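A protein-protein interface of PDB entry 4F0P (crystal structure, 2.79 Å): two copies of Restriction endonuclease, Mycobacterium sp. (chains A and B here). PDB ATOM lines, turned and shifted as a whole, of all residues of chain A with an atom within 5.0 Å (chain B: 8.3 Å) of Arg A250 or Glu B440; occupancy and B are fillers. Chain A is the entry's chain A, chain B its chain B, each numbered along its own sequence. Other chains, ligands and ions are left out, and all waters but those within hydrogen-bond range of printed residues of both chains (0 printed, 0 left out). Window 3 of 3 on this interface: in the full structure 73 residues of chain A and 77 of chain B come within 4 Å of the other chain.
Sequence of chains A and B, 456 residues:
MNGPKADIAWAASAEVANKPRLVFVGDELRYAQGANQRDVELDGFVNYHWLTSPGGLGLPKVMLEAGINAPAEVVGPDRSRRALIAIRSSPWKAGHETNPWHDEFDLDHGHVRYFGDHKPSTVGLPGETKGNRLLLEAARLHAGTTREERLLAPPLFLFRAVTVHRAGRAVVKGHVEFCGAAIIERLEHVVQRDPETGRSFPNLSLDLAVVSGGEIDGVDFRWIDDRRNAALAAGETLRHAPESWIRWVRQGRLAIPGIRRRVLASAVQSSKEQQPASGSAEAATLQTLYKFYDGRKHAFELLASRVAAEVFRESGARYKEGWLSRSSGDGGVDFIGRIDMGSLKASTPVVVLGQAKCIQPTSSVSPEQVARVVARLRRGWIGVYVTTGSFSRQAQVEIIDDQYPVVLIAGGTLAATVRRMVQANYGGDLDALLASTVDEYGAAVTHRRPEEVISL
The backbone carbonyl oxygen (O) of Trp A248 lies within hydrogen-bond range of the guanidinium group (NE) of Arg A150, at 3.5 Å.
NH2 of Arg A150 lies within hydrogen-bond range of O of Arg A250 (3.1 Å).
The guanidinium group of Arg A247 sits at hydrogen-bond distance from the side-chain amide oxygen of Gln A251.
NH2 of Arg B306 is in salt-bridge range of OE1 of Glu B321 (3.5 Å).
NE of Arg A150 is in hydrogen-bond range of O of Val A249, at 2.7 Å.
Printed residues of chain B that touch a printed residue of chain A: Arg B306, Glu B321, Asn B425, Tyr B426 and Glu B440.
Hydrophobic or aromatic side chains of chain B that line the printed part of chain A: Tyr B426.
Printed residues of chain A that touch a printed residue of chain B: Arg A150, Arg A247, Arg A250, Gln A251 and Gly A252.
Among the printed residues, 8 pairs touch across the chains.
Among the printed residues, Asp or Glu carboxylates within 4 Å of a Lys or Arg side-chain nitrogen of the other chain: Arg A247 with Glu B321 (2.6 Å) and Arg A250 with Glu B440 (3.9 Å).
Among the printed residues, pairs that only touch across the chains: Arg A247 with Arg B306, Gln A251 with Asn B425 and Gly A252 with Asn B425.
No position is printed for both chains.
The side-chain amide nitrogen (NE2) of Gln A251 is in hydrogen-bond range of the side-chain carboxylate (OE1) of Glu B440 (2.7 Å).
The side-chain carboxylate (OE2) of Glu B440 is in salt-bridge range of the guanidinium group (NE) of Arg A250 (3.9 Å).
The side-chain carboxylate of Glu B321 lies within salt-bridge range of the guanidinium group of Arg A247 (2.6 Å).
OH of Tyr B426 lies within hydrogen-bond range of O of Gln A251 (3.5 Å).
NH1 of Arg A150 lies within hydrogen-bond range of O of Asn B425.
Printed residues of chain B within 4 Å of Arg A247: Arg B306 (3.9 Å) and Glu B321 (2.6 Å).
Of the printed residues of chain B, Arg A250 touches Glu B440 (3.9 Å).
Printed residues of chain B within 4 Å of Gln A251: Asn B425 (3.6 Å), Tyr B426 (3.5 Å) and Glu B440 (2.7 Å).
Of the printed residues of chain B, Gly A252 touches Asn B425.
Of the printed residues of chain A, Arg B306 touches Arg A247.
Of the printed residues of chain A, Tyr B426 touches Gln A251.
Glu B440 touches just these residues of chain A: Arg A250 (3.9 Å) and Gln A251 (2.7 Å).
The nearest printed residue of chain A that does not touch Glu B440 is Arg A247 (6.2 Å).
The nearest printed residue of chain A that does not touch Asn B425 is Arg A147 (4.3 Å).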
ATOM      1  N   ARG A 147     -25.566   7.459   1.765  1.00  0.00           N
ATOM      2  CA  ARG A 147     -26.521   8.071   2.685  1.00  0.00           C
ATOM      3  C   ARG A 147     -27.955   7.735   2.286  1.00  0.00           C
ATOM      4  O   ARG A 147     -28.829   7.576   3.142  1.00  0.00           O
ATOM      5  CB  ARG A 147     -26.326   9.589   2.729  1.00  0.00           C
ATOM      6  CG  ARG A 147     -27.405  10.333   3.505  1.00  0.00           C
ATOM      7  CD  ARG A 147     -27.162  11.833   3.515  1.00  0.00           C
ATOM      8  NE  ARG A 147     -28.397  12.575   3.761  1.00  0.00           N
ATOM      9  CZ  ARG A 147     -28.809  12.977   4.960  1.00  0.00           C
ATOM     10  NH1 ARG A 147     -28.080  12.719   6.038  1.00  0.00           N
ATOM     11  NH2 ARG A 147     -29.950  13.642   5.078  1.00  0.00           N
ATOM     12  N   ARG A 150     -28.771   4.388   3.639  1.00  0.00           N
ATOM     13  CA  ARG A 150     -28.889   4.486   5.091  1.00  0.00           C
ATOM     14  C   ARG A 150     -30.187   5.168   5.519  1.00  0.00           C
ATOM     15  O   ARG A 150     -30.674   4.948   6.627  1.00  0.00           O
ATOM     16  CB  ARG A 150     -27.674   5.201   5.692  1.00  0.00           C
ATOM     17  CG  ARG A 150     -26.376   4.409   5.572  1.00  0.00           C
ATOM     18  CD  ARG A 150     -25.244   5.038   6.372  1.00  0.00           C
ATOM     19  NE  ARG A 150     -24.814   6.321   5.823  1.00  0.00           N
ATOM     20  CZ  ARG A 150     -23.897   6.457   4.869  1.00  0.00           C
ATOM     21  NH1 ARG A 150     -23.311   5.389   4.347  1.00  0.00           N
ATOM     22  NH2 ARG A 150     -23.566   7.665   4.431  1.00  0.00           N
ATOM     23  N   ILE A 246     -29.025  10.889  12.762  1.00  0.00           N
ATOM     24  CA  ILE A 246     -28.797  11.726  11.588  1.00  0.00           C
ATOM     25  C   ILE A 246     -27.317  11.731  11.225  1.00  0.00           C
ATOM     26  O   ILE A 246     -26.944  11.633  10.047  1.00  0.00           O
ATOM     27  CB  ILE A 246     -29.258  13.174  11.837  1.00  0.00           C
ATOM     28  CG1 ILE A 246     -30.708  13.195  12.324  1.00  0.00           C
ATOM     29  CG2 ILE A 246     -29.098  14.009  10.579  1.00  0.00           C
ATOM     30  CD1 ILE A 246     -31.244  14.582  12.584  1.00  0.00           C
ATOM     31  N   ARG A 247     -26.480  11.843  12.252  1.00  0.00           N
ATOM     32  CA  ARG A 247     -25.038  11.773  12.077  1.00  0.00           C
ATOM     33  C   ARG A 247     -24.646  10.438  11.463  1.00  0.00           C
ATOM     34  O   ARG A 247     -23.802  10.388  10.573  1.00  0.00           O
ATOM     35  CB  ARG A 247     -24.314  11.961  13.411  1.00  0.00           C
ATOM     36  CG  ARG A 247     -22.806  11.841  13.295  1.00  0.00           C
ATOM     37  CD  ARG A 247     -22.123  11.846  14.650  1.00  0.00           C
ATOM     38  NE  ARG A 247     -20.707  11.514  14.526  1.00  0.00           N
ATOM     39  CZ  ARG A 247     -19.869  11.395  15.553  1.00  0.00           C
ATOM     40  NH1 ARG A 247     -20.302  11.582  16.792  1.00  0.00           N
ATOM     41  NH2 ARG A 247     -18.598  11.089  15.337  1.00  0.00           N
ATOM     42  N   TRP A 248     -25.260   9.357  11.936  1.00  0.00           N
ATOM     43  CA  TRP A 248     -24.976   8.039  11.383  1.00  0.00           C
ATOM     44  C   TRP A 248     -25.353   7.953   9.911  1.00  0.00           C
ATOM     45  O   TRP A 248     -24.588   7.437   9.098  1.00  0.00           O
ATOM     46  CB  TRP A 248     -25.697   6.935  12.154  1.00  0.00           C
ATOM     47  CG  TRP A 248     -25.732   5.654  11.378  1.00  0.00           C
ATOM     48  CD1 TRP A 248     -24.683   4.819  11.129  1.00  0.00           C
ATOM     49  CD2 TRP A 248     -26.872   5.072  10.732  1.00  0.00           C
ATOM     50  NE1 TRP A 248     -25.098   3.748  10.373  1.00  0.00           N
ATOM     51  CE2 TRP A 248     -26.438   3.880  10.118  1.00  0.00           C
ATOM     52  CE3 TRP A 248     -28.216   5.438  10.618  1.00  0.00           C
ATOM     53  CZ2 TRP A 248     -27.301   3.053   9.400  1.00  0.00           C
ATOM     54  CZ3 TRP A 248     -29.072   4.616   9.906  1.00  0.00           C
ATOM     55  CH2 TRP A 248     -28.611   3.438   9.306  1.00  0.00           C
ATOM     56  N   VAL A 249     -26.541   8.449   9.576  1.00  0.00           N
ATOM     57  CA  VAL A 249     -27.016   8.450   8.199  1.00  0.00           C
ATOM     58  C   VAL A 249     -26.046   9.217   7.308  1.00  0.00           C
ATOM     59  O   VAL A 249     -25.748   8.793   6.191  1.00  0.00           O
ATOM     60  CB  VAL A 249     -28.426   9.067   8.083  1.00  0.00           C
ATOM     61  CG1 VAL A 249     -28.868   9.120   6.630  1.00  0.00           C
ATOM     62  CG2 VAL A 249     -29.423   8.274   8.911  1.00  0.00           C
ATOM     63  N   ARG A 250     -25.537  10.337   7.814  1.00  0.00           N
ATOM     64  CA  ARG A 250     -24.598  11.144   7.043  1.00  0.00           C
ATOM     65  C   ARG A 250     -23.235  10.464   6.871  1.00  0.00           C
ATOM     66  O   ARG A 250     -22.727  10.346   5.756  1.00  0.00           O
ATOM     67  CB  ARG A 250     -24.422  12.525   7.683  1.00  0.00           C
ATOM     68  CG  ARG A 250     -23.515  13.457   6.892  1.00  0.00           C
ATOM     69  CD  ARG A 250     -23.425  14.842   7.519  1.00  0.00           C
ATOM     70  NE  ARG A 250     -22.751  14.829   8.814  1.00  0.00           N
ATOM     71  CZ  ARG A 250     -23.380  14.870   9.986  1.00  0.00           C
ATOM     72  NH1 ARG A 250     -24.705  14.932  10.031  1.00  0.00           N
ATOM     73  NH2 ARG A 250     -22.683  14.854  11.115  1.00  0.00           N
ATOM     74  N   GLN A 251     -22.655  10.010   7.978  1.00  0.00           N
ATOM     75  CA  GLN A 251     -21.282   9.509   7.985  1.00  0.00           C
ATOM     76  C   GLN A 251     -21.165   8.003   7.762  1.00  0.00           C
ATOM     77  O   GLN A 251     -20.224   7.538   7.122  1.00  0.00           O
ATOM     78  CB  GLN A 251     -20.580   9.898   9.289  1.00  0.00           C
ATOM     79  CG  GLN A 251     -20.371  11.395   9.453  1.00  0.00           C
ATOM     80  CD  GLN A 251     -19.635  11.739  10.732  1.00  0.00           C
ATOM     81  OE1 GLN A 251     -19.439  10.885  11.595  1.00  0.00           O
ATOM     82  NE2 GLN A 251     -19.223  12.996  10.858  1.00  0.00           N
ATOM     83  N   GLY A 252     -22.114   7.244   8.300  1.00  0.00           N
ATOM     84  CA  GLY A 252     -22.103   5.801   8.140  1.00  0.00           C
ATOM     85  C   GLY A 252     -21.481   5.086   9.322  1.00  0.00           C
ATOM     86  O   GLY A 252     -21.806   5.373  10.474  1.00  0.00           O
ATOM     87  N   HIS B 298      -4.482  19.118  11.308  1.00  0.00           N
ATOM     88  CA  HIS B 298      -5.509  18.682  12.247  1.00  0.00           C
ATOM     89  C   HIS B 298      -6.647  17.935  11.559  1.00  0.00           C
ATOM     90  O   HIS B 298      -7.274  17.054  12.156  1.00  0.00           O
ATOM     91  CB  HIS B 298      -6.038  19.882  13.029  1.00  0.00           C
ATOM     92  CG  HIS B 298      -4.957  20.727  13.625  1.00  0.00           C
ATOM     93  ND1 HIS B 298      -4.443  20.501  14.883  1.00  0.00           N
ATOM     94  CD2 HIS B 298      -4.277  21.786  13.126  1.00  0.00           C
ATOM     95  CE1 HIS B 298      -3.500  21.389  15.137  1.00  0.00           C
ATOM     96  NE2 HIS B 298      -3.380  22.182  14.088  1.00  0.00           N
ATOM     97  N   ALA B 299      -6.909  18.290  10.305  1.00  0.00           N
ATOM     98  CA  ALA B 299      -7.880  17.564   9.495  1.00  0.00           C
ATOM     99  C   ALA B 299      -7.361  16.154   9.251  1.00  0.00           C
ATOM    100  O   ALA B 299      -8.118  15.177   9.277  1.00  0.00           O
ATOM    101  CB  ALA B 299      -8.110  18.281   8.178  1.00  0.00           C
ATOM    102  N   LEU B 302      -7.889  14.209  12.415  1.00  0.00           N
ATOM    103  CA  LEU B 302      -9.251  13.685  12.486  1.00  0.00           C
ATOM    104  C   LEU B 302      -9.392  12.448  11.599  1.00  0.00           C
ATOM    105  O   LEU B 302      -9.919  11.405  12.023  1.00  0.00           O
ATOM    106  CB  LEU B 302     -10.254  14.756  12.056  1.00  0.00           C
ATOM    107  CG  LEU B 302     -11.730  14.355  12.057  1.00  0.00           C
ATOM    108  CD1 LEU B 302     -12.159  13.913  13.447  1.00  0.00           C
ATOM    109  CD2 LEU B 302     -12.603  15.501  11.561  1.00  0.00           C
ATOM    110  N   ARG B 306     -10.238   8.477  12.502  1.00  0.00           N
ATOM    111  CA  ARG B 306     -11.203   7.611  11.822  1.00  0.00           C
ATOM    112  C   ARG B 306     -10.572   6.309  11.308  1.00  0.00           C
ATOM    113  O   ARG B 306     -11.114   5.214  11.514  1.00  0.00           O
ATOM    114  CB  ARG B 306     -11.876   8.365  10.672  1.00  0.00           C
ATOM    115  CG  ARG B 306     -12.621   9.622  11.104  1.00  0.00           C
ATOM    116  CD  ARG B 306     -13.760   9.291  12.056  1.00  0.00           C
ATOM    117  NE  ARG B 306     -14.567  10.465  12.380  1.00  0.00           N
ATOM    118  CZ  ARG B 306     -14.444  11.172  13.499  1.00  0.00           C
ATOM    119  NH1 ARG B 306     -13.545  10.826  14.410  1.00  0.00           N
ATOM    120  NH2 ARG B 306     -15.225  12.225  13.707  1.00  0.00           N
ATOM    121  N   GLU B 321     -14.789   6.428  19.966  1.00  0.00           N
ATOM    122  CA  GLU B 321     -14.290   7.718  19.499  1.00  0.00           C
ATOM    123  C   GLU B 321     -14.126   8.704  20.647  1.00  0.00           C
ATOM    124  O   GLU B 321     -15.093   9.040  21.334  1.00  0.00           O
ATOM    125  CB  GLU B 321     -15.232   8.310  18.452  1.00  0.00           C
ATOM    126  CG  GLU B 321     -14.911   9.749  18.088  1.00  0.00           C
ATOM    127  CD  GLU B 321     -16.003  10.397  17.262  1.00  0.00           C
ATOM    128  OE1 GLU B 321     -15.929  11.624  17.036  1.00  0.00           O
ATOM    129  OE2 GLU B 321     -16.936   9.682  16.839  1.00  0.00           O
ATOM    130  N   LEU B 324      -9.829  15.114  19.737  1.00  0.00           N
ATOM    131  CA  LEU B 324      -8.546  15.649  19.303  1.00  0.00           C
ATOM    132  C   LEU B 324      -7.990  16.552  20.394  1.00  0.00           C
ATOM    133  O   LEU B 324      -8.723  17.335  20.996  1.00  0.00           O
ATOM    134  CB  LEU B 324      -8.686  16.424  17.991  1.00  0.00           C
ATOM    135  CG  LEU B 324      -8.557  15.645  16.678  1.00  0.00           C
ATOM    136  CD1 LEU B 324      -9.650  14.595  16.531  1.00  0.00           C
ATOM    137  CD2 LEU B 324      -8.571  16.600  15.494  1.00  0.00           C
ATOM    138  N   ASN B 425     -19.187   3.692   2.573  1.00  0.00           N
ATOM    139  CA  ASN B 425     -19.993   4.693   3.273  1.00  0.00           C
ATOM    140  C   ASN B 425     -20.386   5.908   2.434  1.00  0.00           C
ATOM    141  O   ASN B 425     -21.424   6.524   2.680  1.00  0.00           O
ATOM    142  CB  ASN B 425     -19.292   5.154   4.556  1.00  0.00           C
ATOM    143  CG  ASN B 425     -19.040   4.013   5.525  1.00  0.00           C
ATOM    144  OD1 ASN B 425     -19.941   3.581   6.245  1.00  0.00           O
ATOM    145  ND2 ASN B 425     -17.806   3.522   5.550  1.00  0.00           N
ATOM    146  N   TYR B 426     -19.561   6.250   1.450  1.00  0.00           N
ATOM    147  CA  TYR B 426     -19.794   7.452   0.652  1.00  0.00           C
ATOM    148  C   TYR B 426     -20.000   7.157  -0.833  1.00  0.00           C
ATOM    149  O   TYR B 426     -20.019   8.071  -1.659  1.00  0.00           O
ATOM    150  CB  TYR B 426     -18.652   8.452   0.848  1.00  0.00           C
ATOM    151  CG  TYR B 426     -18.496   8.903   2.282  1.00  0.00           C
ATOM    152  CD1 TYR B 426     -19.212   9.988   2.771  1.00  0.00           C
ATOM    153  CD2 TYR B 426     -17.643   8.236   3.151  1.00  0.00           C
ATOM    154  CE1 TYR B 426     -19.077  10.400   4.085  1.00  0.00           C
ATOM    155  CE2 TYR B 426     -17.502   8.640   4.466  1.00  0.00           C
ATOM    156  CZ  TYR B 426     -18.221   9.723   4.927  1.00  0.00           C
ATOM    157  OH  TYR B 426     -18.083  10.128   6.235  1.00  0.00           O
ATOM    158  N   ALA B 432     -16.259  13.801  -0.348  1.00  0.00           N
ATOM    159  CA  ALA B 432     -17.167  13.886   0.788  1.00  0.00           C
ATOM    160  C   ALA B 432     -16.420  13.645   2.093  1.00  0.00           C
ATOM    161  O   ALA B 432     -16.609  14.365   3.073  1.00  0.00           O
ATOM    162  CB  ALA B 432     -18.302  12.886   0.633  1.00  0.00           C
ATOM    163  N   LEU B 433     -15.565  12.627   2.090  1.00  0.00           N
ATOM    164  CA  LEU B 433     -14.772  12.281   3.262  1.00  0.00           C
ATOM    165  C   LEU B 433     -13.771  13.382   3.596  1.00  0.00           C
ATOM    166  O   LEU B 433     -13.662  13.811   4.750  1.00  0.00           O
ATOM    167  CB  LEU B 433     -14.042  10.956   3.031  1.00  0.00           C
ATOM    168  CG  LEU B 433     -13.192  10.434   4.191  1.00  0.00           C
ATOM    169  CD1 LEU B 433     -14.034  10.279   5.448  1.00  0.00           C
ATOM    170  CD2 LEU B 433     -12.537   9.115   3.819  1.00  0.00           C
ATOM    171  N   LEU B 434     -13.044  13.837   2.578  1.00  0.00           N
ATOM    172  CA  LEU B 434     -12.048  14.888   2.764  1.00  0.00           C
ATOM    173  C   LEU B 434     -12.680  16.160   3.330  1.00  0.00           C
ATOM    174  O   LEU B 434     -12.178  16.746   4.296  1.00  0.00           O
ATOM    175  CB  LEU B 434     -11.341  15.182   1.442  1.00  0.00           C
ATOM    176  CG  LEU B 434     -10.639  13.981   0.800  1.00  0.00           C
ATOM    177  CD1 LEU B 434     -10.063  14.347  -0.559  1.00  0.00           C
ATOM    178  CD2 LEU B 434      -9.553  13.439   1.716  1.00  0.00           C
ATOM    179  N   ALA B 435     -13.793  16.571   2.733  1.00  0.00           N
ATOM    180  CA  ALA B 435     -14.521  17.746   3.197  1.00  0.00           C
ATOM    181  C   ALA B 435     -15.071  17.519   4.600  1.00  0.00           C
ATOM    182  O   ALA B 435     -15.194  18.458   5.388  1.00  0.00           O
ATOM    183  CB  ALA B 435     -15.645  18.091   2.231  1.00  0.00           C
ATOM    184  N   SER B 436     -15.401  16.268   4.909  1.00  0.00           N
ATOM    185  CA  SER B 436     -15.877  15.915   6.240  1.00  0.00           C
ATOM    186  C   SER B 436     -14.781  16.130   7.277  1.00  0.00           C
ATOM    187  O   SER B 436     -15.047  16.607   8.381  1.00  0.00           O
ATOM    188  CB  SER B 436     -16.366  14.466   6.278  1.00  0.00           C
ATOM    189  OG  SER B 436     -17.463  14.275   5.400  1.00  0.00           O
ATOM    190  N   THR B 437     -13.549  15.781   6.920  1.00  0.00           N
ATOM    191  CA  THR B 437     -12.421  15.972   7.830  1.00  0.00           C
ATOM    192  C   THR B 437     -12.012  17.440   7.930  1.00  0.00           C
ATOM    193  O   THR B 437     -11.498  17.877   8.959  1.00  0.00           O
ATOM    194  CB  THR B 437     -11.197  15.130   7.420  1.00  0.00           C
ATOM    195  OG1 THR B 437     -10.812  15.459   6.079  1.00  0.00           O
ATOM    196  CG2 THR B 437     -11.520  13.649   7.502  1.00  0.00           C
ATOM    197  N   VAL B 438     -12.242  18.197   6.862  1.00  0.00           N
ATOM    198  CA  VAL B 438     -11.911  19.621   6.864  1.00  0.00           C
ATOM    199  C   VAL B 438     -12.927  20.446   7.658  1.00  0.00           C
ATOM    200  O   VAL B 438     -12.569  21.411   8.334  1.00  0.00           O
ATOM    201  CB  VAL B 438     -11.790  20.174   5.424  1.00  0.00           C
ATOM    202  CG1 VAL B 438     -11.635  21.689   5.429  1.00  0.00           C
ATOM    203  CG2 VAL B 438     -10.617  19.529   4.711  1.00  0.00           C
ATOM    204  N   ASP B 439     -14.194  20.054   7.589  1.00  0.00           N
ATOM    205  CA  ASP B 439     -15.265  20.845   8.186  1.00  0.00           C
ATOM    206  C   ASP B 439     -15.607  20.452   9.624  1.00  0.00           C
ATOM    207  O   ASP B 439     -16.340  21.169  10.305  1.00  0.00           O
ATOM    208  CB  ASP B 439     -16.524  20.774   7.314  1.00  0.00           C
ATOM    209  N   GLU B 440     -15.079  19.324  10.087  1.00  0.00           N
ATOM    210  CA  GLU B 440     -15.454  18.803  11.401  1.00  0.00           C
ATOM    211  C   GLU B 440     -14.279  18.626  12.364  1.00  0.00           C
ATOM    212  O   GLU B 440     -14.435  18.026  13.428  1.00  0.00           O
ATOM    213  CB  GLU B 440     -16.204  17.475  11.255  1.00  0.00           C
ATOM    214  CG  GLU B 440     -17.490  17.560  10.443  1.00  0.00           C
ATOM    215  CD  GLU B 440     -18.134  16.201  10.223  1.00  0.00           C
ATOM    216  OE1 GLU B 440     -17.581  15.191  10.712  1.00  0.00           O
ATOM    217  OE2 GLU B 440     -19.192  16.142   9.559  1.00  0.00           O
ATOM    218  N   TYR B 441     -13.111  19.147  12.002  1.00  0.00           N
ATOM    219  CA  TYR B 441     -11.926  18.970  12.838  1.00  0.00           C
ATOM    220  C   TYR B 441     -11.843  20.004  13.959  1.00  0.00           C
ATOM    221  O   TYR B 441     -10.974  19.921  14.827  1.00  0.00           O
ATOM    222  CB  TYR B 441     -10.649  18.998  11.991  1.00  0.00           C
ATOM    223  CG  TYR B 441     -10.137  20.386  11.673  1.00  0.00           C
ATOM    224  CD1 TYR B 441     -10.625  21.096  10.587  1.00  0.00           C
ATOM    225  CD2 TYR B 441      -9.157  20.982  12.457  1.00  0.00           C
ATOM    226  CE1 TYR B 441     -10.155  22.363  10.293  1.00  0.00           C
ATOM    227  CE2 TYR B 441      -8.681  22.246  12.171  1.00  0.00           C
ATOM    228  CZ  TYR B 441      -9.183  22.932  11.088  1.00  0.00           C
ATOM    229  OH  TYR B 441      -8.709  24.192  10.804  1.00  0.00           O
ATOM    230  N   GLY B 442     -12.747  20.979  13.935  1.00  0.00           N
ATOM    231  CA  GLY B 442     -12.753  22.029  14.936  1.00  0.00           C
ATOM    232  C   GLY B 442     -13.605  21.695  16.144  1.00  0.00           C
ATOM    233  O   GLY B 442     -13.272  22.066  17.271  1.00  0.00           O
ATOM    234  N   ALA B 443     -14.704  20.985  15.910  1.00  0.00           N
ATOM    235  CA  ALA B 443     -15.649  20.654  16.972  1.00  0.00           C
ATOM    236  C   ALA B 443     -15.354  19.300  17.615  1.00  0.00           C
ATOM    237  O   ALA B 443     -16.128  18.815  18.442  1.00  0.00           O
ATOM    238  CB  ALA B 443     -17.076  20.691  16.439  1.00  0.00           C
ATOM    239  N   ALA B 444     -14.236  18.693  17.231  1.00  0.00           N
ATOM    240  CA  ALA B 444     -13.835  17.404  17.787  1.00  0.00           C
ATOM    241  C   ALA B 444     -12.717  17.584  18.807  1.00  0.00           C
ATOM    242  O   ALA B 444     -12.232  16.616  19.397  1.00  0.00           O
ATOM    243  CB  ALA B 444     -13.398  16.462  16.677  1.00  0.00           C
ATOM    244  N   VAL B 445     -12.317  18.834  19.013  1.00  0.00           N
ATOM    245  CA  VAL B 445     -11.205  19.155  19.896  1.00  0.00           C
ATOM    246  C   VAL B 445     -11.661  19.473  21.317  1.00  0.00           C
ATOM    247  O   VAL B 445     -12.466  20.379  21.532  1.00  0.00           O
ATOM    248  CB  VAL B 445     -10.400  20.348  19.354  1.00  0.00           C
ATOM    249  CG1 VAL B 445      -9.369  20.803  20.372  1.00  0.00           C
ATOM    250  CG2 VAL B 445      -9.743  19.981  18.034  1.00  0.00           C
